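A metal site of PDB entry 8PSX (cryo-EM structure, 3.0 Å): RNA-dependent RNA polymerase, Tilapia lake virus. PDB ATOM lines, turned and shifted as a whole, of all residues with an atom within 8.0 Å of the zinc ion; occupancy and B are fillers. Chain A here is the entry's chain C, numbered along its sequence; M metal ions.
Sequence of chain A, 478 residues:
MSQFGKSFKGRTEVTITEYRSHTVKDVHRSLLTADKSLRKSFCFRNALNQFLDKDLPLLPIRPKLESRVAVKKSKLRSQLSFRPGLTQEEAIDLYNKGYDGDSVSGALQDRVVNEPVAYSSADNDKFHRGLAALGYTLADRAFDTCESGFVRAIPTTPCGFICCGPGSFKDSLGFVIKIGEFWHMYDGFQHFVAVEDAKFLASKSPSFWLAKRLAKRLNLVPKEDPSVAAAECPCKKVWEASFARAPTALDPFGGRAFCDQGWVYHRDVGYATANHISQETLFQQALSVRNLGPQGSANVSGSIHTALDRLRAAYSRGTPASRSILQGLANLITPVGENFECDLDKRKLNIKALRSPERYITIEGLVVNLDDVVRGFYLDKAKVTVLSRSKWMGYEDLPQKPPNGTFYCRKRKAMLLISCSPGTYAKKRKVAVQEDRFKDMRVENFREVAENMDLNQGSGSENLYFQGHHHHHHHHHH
The zinc ion is bound by a ring nitrogen (NE2) of His 191 (2.0 Å), a ring nitrogen (ND1) of His 184 (2.0 Å), the side-chain sulfur of Cys 233 (2.3 Å) and the side-chain sulfur of Cys 235 (2.3 Å). The zinc ion has four donor atoms within binding distance.
O of Ile 177 sits at hydrogen-bond distance from N of His 184, 2.9 Å away.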
ATOM      1  N   PHE A 175     -15.549  26.130  11.884  1.00  0.00           N
ATOM      2  CA  PHE A 175     -15.857  24.837  11.302  1.00  0.00           C
ATOM      3  C   PHE A 175     -16.596  25.015   9.984  1.00  0.00           C
ATOM      4  O   PHE A 175     -17.437  25.902   9.832  1.00  0.00           O
ATOM      5  CB  PHE A 175     -16.668  23.956  12.269  1.00  0.00           C
ATOM      6  CG  PHE A 175     -18.125  24.319  12.362  1.00  0.00           C
ATOM      7  CD1 PHE A 175     -19.038  23.830  11.432  1.00  0.00           C
ATOM      8  CD2 PHE A 175     -18.589  25.120  13.389  1.00  0.00           C
ATOM      9  CE1 PHE A 175     -20.370  24.155  11.522  1.00  0.00           C
ATOM     10  CE2 PHE A 175     -19.921  25.445  13.479  1.00  0.00           C
ATOM     11  CZ  PHE A 175     -20.822  24.962  12.543  1.00  0.00           C
ATOM     12  N   ILE A 177     -18.892  22.747   7.257  1.00  0.00           N
ATOM     13  CA  ILE A 177     -19.691  21.535   7.145  1.00  0.00           C
ATOM     14  C   ILE A 177     -20.496  21.629   5.858  1.00  0.00           C
ATOM     15  O   ILE A 177     -20.722  22.718   5.315  1.00  0.00           O
ATOM     16  CB  ILE A 177     -20.604  21.342   8.384  1.00  0.00           C
ATOM     17  CG1 ILE A 177     -21.518  20.118   8.220  1.00  0.00           C
ATOM     18  CG2 ILE A 177     -21.412  22.611   8.642  1.00  0.00           C
ATOM     19  CD1 ILE A 177     -22.556  19.971   9.320  1.00  0.00           C
ATOM     20  N   ILE A 179     -24.093  20.847   4.143  1.00  0.00           N
ATOM     21  CA  ILE A 179     -25.516  20.578   4.356  1.00  0.00           C
ATOM     22  C   ILE A 179     -26.191  20.608   2.996  1.00  0.00           C
ATOM     23  O   ILE A 179     -26.099  21.611   2.273  1.00  0.00           O
ATOM     24  CB  ILE A 179     -26.152  21.602   5.310  1.00  0.00           C
ATOM     25  CG1 ILE A 179     -25.470  21.556   6.670  1.00  0.00           C
ATOM     26  CG2 ILE A 179     -27.647  21.328   5.459  1.00  0.00           C
ATOM     27  CD1 ILE A 179     -24.682  22.808   7.005  1.00  0.00           C
ATOM     28  N   PHE A 182     -24.837  22.773  -0.066  1.00  0.00           N
ATOM     29  CA  PHE A 182     -24.143  24.014   0.282  1.00  0.00           C
ATOM     30  C   PHE A 182     -23.131  23.733   1.375  1.00  0.00           C
ATOM     31  O   PHE A 182     -23.221  22.743   2.099  1.00  0.00           O
ATOM     32  CB  PHE A 182     -25.127  25.096   0.735  1.00  0.00           C
ATOM     33  CG  PHE A 182     -25.877  25.748  -0.394  1.00  0.00           C
ATOM     34  CD1 PHE A 182     -26.865  25.064  -1.073  1.00  0.00           C
ATOM     35  CD2 PHE A 182     -25.575  27.039  -0.788  1.00  0.00           C
ATOM     36  CE1 PHE A 182     -27.552  25.663  -2.112  1.00  0.00           C
ATOM     37  CE2 PHE A 182     -26.253  27.636  -1.827  1.00  0.00           C
ATOM     38  CZ  PHE A 182     -27.241  26.952  -2.492  1.00  0.00           C
ATOM     39  N   TRP A 183     -22.147  24.629   1.492  1.00  0.00           N
ATOM     40  CA  TRP A 183     -21.082  24.523   2.489  1.00  0.00           C
ATOM     41  C   TRP A 183     -21.244  25.681   3.473  1.00  0.00           C
ATOM     42  O   TRP A 183     -21.020  26.833   3.106  1.00  0.00           O
ATOM     43  CB  TRP A 183     -19.708  24.546   1.830  1.00  0.00           C
ATOM     44  CG  TRP A 183     -19.393  23.328   1.034  1.00  0.00           C
ATOM     45  CD1 TRP A 183     -19.644  23.125  -0.288  1.00  0.00           C
ATOM     46  CD2 TRP A 183     -18.751  22.128   1.509  1.00  0.00           C
ATOM     47  NE1 TRP A 183     -19.200  21.874  -0.674  1.00  0.00           N
ATOM     48  CE2 TRP A 183     -18.649  21.248   0.412  1.00  0.00           C
ATOM     49  CE3 TRP A 183     -18.259  21.727   2.756  1.00  0.00           C
ATOM     50  CZ2 TRP A 183     -18.082  19.988   0.536  1.00  0.00           C
ATOM     51  CZ3 TRP A 183     -17.690  20.476   2.859  1.00  0.00           C
ATOM     52  CH2 TRP A 183     -17.603  19.620   1.756  1.00  0.00           C
ATOM     53  N   HIS A 184     -21.610  25.370   4.708  1.00  0.00           N
ATOM     54  CA  HIS A 184     -21.741  26.367   5.747  1.00  0.00           C
ATOM     55  C   HIS A 184     -20.444  26.475   6.530  1.00  0.00           C
ATOM     56  O   HIS A 184     -19.938  25.471   7.043  1.00  0.00           O
ATOM     57  CB  HIS A 184     -22.888  26.025   6.701  1.00  0.00           C
ATOM     58  CG  HIS A 184     -24.236  25.971   6.041  1.00  0.00           C
ATOM     59  ND1 HIS A 184     -25.349  26.583   6.581  1.00  0.00           N
ATOM     60  CD2 HIS A 184     -24.651  25.370   4.909  1.00  0.00           C
ATOM     61  CE1 HIS A 184     -26.383  26.360   5.800  1.00  0.00           C
ATOM     62  NE2 HIS A 184     -25.987  25.630   4.776  1.00  0.00           N
ATOM     63  N   MET A 185     -19.909  27.695   6.614  1.00  0.00           N
ATOM     64  CA  MET A 185     -18.730  27.983   7.421  1.00  0.00           C
ATOM     65  C   MET A 185     -19.142  28.890   8.560  1.00  0.00           C
ATOM     66  O   MET A 185     -19.648  29.993   8.322  1.00  0.00           O
ATOM     67  CB  MET A 185     -17.641  28.660   6.585  1.00  0.00           C
ATOM     68  CG  MET A 185     -17.178  27.862   5.381  1.00  0.00           C
ATOM     69  SD  MET A 185     -17.004  28.891   3.923  1.00  0.00           S
ATOM     70  CE  MET A 185     -18.680  28.875   3.299  1.00  0.00           C
ATOM     71  N   TYR A 186     -18.922  28.447   9.797  1.00  0.00           N
ATOM     72  CA  TYR A 186     -19.265  29.231  10.979  1.00  0.00           C
ATOM     73  C   TYR A 186     -18.036  29.353  11.869  1.00  0.00           C
ATOM     74  O   TYR A 186     -17.398  28.350  12.184  1.00  0.00           O
ATOM     75  CB  TYR A 186     -20.436  28.609  11.741  1.00  0.00           C
ATOM     76  CG  TYR A 186     -20.887  29.413  12.938  1.00  0.00           C
ATOM     77  CD1 TYR A 186     -20.831  30.793  12.937  1.00  0.00           C
ATOM     78  CD2 TYR A 186     -21.386  28.780  14.076  1.00  0.00           C
ATOM     79  CE1 TYR A 186     -21.255  31.532  14.024  1.00  0.00           C
ATOM     80  CE2 TYR A 186     -21.812  29.505  15.163  1.00  0.00           C
ATOM     81  CZ  TYR A 186     -21.737  30.876  15.140  1.00  0.00           C
ATOM     82  OH  TYR A 186     -22.162  31.608  16.234  1.00  0.00           O
ATOM     83  N   HIS A 191     -21.099  33.849   9.975  1.00  0.00           N
ATOM     84  CA  HIS A 191     -21.530  32.612   9.338  1.00  0.00           C
ATOM     85  C   HIS A 191     -21.791  32.895   7.872  1.00  0.00           C
ATOM     86  O   HIS A 191     -22.573  33.781   7.536  1.00  0.00           O
ATOM     87  CB  HIS A 191     -22.792  32.048  10.010  1.00  0.00           C
ATOM     88  CG  HIS A 191     -23.500  31.017   9.185  1.00  0.00           C
ATOM     89  ND1 HIS A 191     -24.431  31.348   8.223  1.00  0.00           N
ATOM     90  CD2 HIS A 191     -23.418  29.668   9.189  1.00  0.00           C
ATOM     91  CE1 HIS A 191     -24.896  30.249   7.657  1.00  0.00           C
ATOM     92  NE2 HIS A 191     -24.294  29.210   8.225  1.00  0.00           N
ATOM     93  N   PHE A 192     -21.150  32.117   6.996  1.00  0.00           N
ATOM     94  CA  PHE A 192     -21.294  32.268   5.559  1.00  0.00           C
ATOM     95  C   PHE A 192     -21.632  30.925   4.931  1.00  0.00           C
ATOM     96  O   PHE A 192     -21.510  29.873   5.553  1.00  0.00           O
ATOM     97  CB  PHE A 192     -20.019  32.842   4.916  1.00  0.00           C
ATOM     98  CG  PHE A 192     -19.646  34.213   5.419  1.00  0.00           C
ATOM     99  CD1 PHE A 192     -20.619  35.142   5.750  1.00  0.00           C
ATOM    100  CD2 PHE A 192     -18.317  34.567   5.564  1.00  0.00           C
ATOM    101  CE1 PHE A 192     -20.268  36.398   6.210  1.00  0.00           C
ATOM    102  CE2 PHE A 192     -17.957  35.813   6.031  1.00  0.00           C
ATOM    103  CZ  PHE A 192     -18.942  36.731   6.347  1.00  0.00           C
ATOM    104  N   VAL A 193     -22.065  30.991   3.672  1.00  0.00           N
ATOM    105  CA  VAL A 193     -22.444  29.816   2.905  1.00  0.00           C
ATOM    106  C   VAL A 193     -21.795  29.907   1.531  1.00  0.00           C
ATOM    107  O   VAL A 193     -21.684  31.000   0.955  1.00  0.00           O
ATOM    108  CB  VAL A 193     -23.982  29.703   2.772  1.00  0.00           C
ATOM    109  CG1 VAL A 193     -24.365  28.847   1.590  1.00  0.00           C
ATOM    110  CG2 VAL A 193     -24.579  29.138   4.056  1.00  0.00           C
ATOM    111  N   ALA A 230     -28.688  29.502   1.609  1.00  0.00           N
ATOM    112  CA  ALA A 230     -29.315  28.216   1.854  1.00  0.00           C
ATOM    113  C   ALA A 230     -30.568  28.397   2.702  1.00  0.00           C
ATOM    114  O   ALA A 230     -30.766  29.429   3.346  1.00  0.00           O
ATOM    115  CB  ALA A 230     -28.341  27.258   2.556  1.00  0.00           C
ATOM    116  N   GLU A 232     -32.024  25.928   5.230  1.00  0.00           N
ATOM    117  CA  GLU A 232     -31.908  25.469   6.607  1.00  0.00           C
ATOM    118  C   GLU A 232     -30.442  25.458   7.009  1.00  0.00           C
ATOM    119  O   GLU A 232     -29.607  24.834   6.340  1.00  0.00           O
ATOM    120  CB  GLU A 232     -32.505  24.073   6.768  1.00  0.00           C
ATOM    121  CG  GLU A 232     -34.020  24.030   6.597  1.00  0.00           C
ATOM    122  CD  GLU A 232     -34.755  24.628   7.781  1.00  0.00           C
ATOM    123  OE1 GLU A 232     -35.012  23.880   8.752  1.00  0.00           O
ATOM    124  OE2 GLU A 232     -35.078  25.830   7.733  1.00  0.00           O
ATOM    125  N   CYS A 233     -30.120  26.158   8.097  1.00  0.00           N
ATOM    126  CA  CYS A 233     -28.742  26.325   8.572  1.00  0.00           C
ATOM    127  C   CYS A 233     -28.691  25.952  10.045  1.00  0.00           C
ATOM    128  O   CYS A 233     -28.757  26.816  10.922  1.00  0.00           O
ATOM    129  CB  CYS A 233     -28.253  27.745   8.341  1.00  0.00           C
ATOM    130  SG  CYS A 233     -26.669  28.129   9.140  1.00  0.00           S
ATOM    131  N   PRO A 234     -28.577  24.651  10.363  1.00  0.00           N
ATOM    132  CA  PRO A 234     -28.513  24.243  11.772  1.00  0.00           C
ATOM    133  C   PRO A 234     -27.158  24.498  12.428  1.00  0.00           C
ATOM    134  O   PRO A 234     -26.880  23.989  13.513  1.00  0.00           O
ATOM    135  CB  PRO A 234     -28.806  22.739  11.694  1.00  0.00           C
ATOM    136  CG  PRO A 234     -28.298  22.351  10.350  1.00  0.00           C
ATOM    137  CD  PRO A 234     -28.719  23.496   9.470  1.00  0.00           C
ATOM    138  N   CYS A 235     -26.318  25.306  11.775  1.00  0.00           N
ATOM    139  CA  CYS A 235     -24.953  25.512  12.259  1.00  0.00           C
ATOM    140  C   CYS A 235     -24.951  25.853  13.744  1.00  0.00           C
ATOM    141  O   CYS A 235     -24.206  25.243  14.528  1.00  0.00           O
ATOM    142  CB  CYS A 235     -24.272  26.618  11.452  1.00  0.00           C
ATOM    143  SG  CYS A 235     -23.455  26.035   9.971  1.00  0.00           S
ATOM    144  N   LYS A 236     -25.784  26.816  14.156  1.00  0.00           N
ATOM    145  CA  LYS A 236     -25.799  27.230  15.552  1.00  0.00           C
ATOM    146  C   LYS A 236     -25.879  26.019  16.469  1.00  0.00           C
ATOM    147  O   LYS A 236     -25.057  25.863  17.378  1.00  0.00           O
ATOM    148  CB  LYS A 236     -26.973  28.173  15.798  1.00  0.00           C
ATOM    149  CG  LYS A 236     -26.868  29.512  15.087  1.00  0.00           C
ATOM    150  CD  LYS A 236     -28.114  30.345  15.334  1.00  0.00           C
ATOM    151  CE  LYS A 236     -27.977  31.743  14.753  1.00  0.00           C
ATOM    152  NZ  LYS A 236     -29.245  32.516  14.869  1.00  0.00           N
ATOM    153  N   VAL A 238     -25.087  22.834  15.991  1.00  0.00           N
ATOM    154  CA  VAL A 238     -23.861  22.046  16.016  1.00  0.00           C
ATOM    155  C   VAL A 238     -22.731  22.842  16.653  1.00  0.00           C
ATOM    156  O   VAL A 238     -21.807  22.268  17.240  1.00  0.00           O
ATOM    157  CB  VAL A 238     -23.496  21.552  14.602  1.00  0.00           C
ATOM    158  CG1 VAL A 238     -24.668  20.806  13.983  1.00  0.00           C
ATOM    159  CG2 VAL A 238     -23.083  22.692  13.704  1.00  0.00           C
HETATM  160 ZN    ZN M   1     -24.689  27.213   8.410  1.00  0.00          ZN
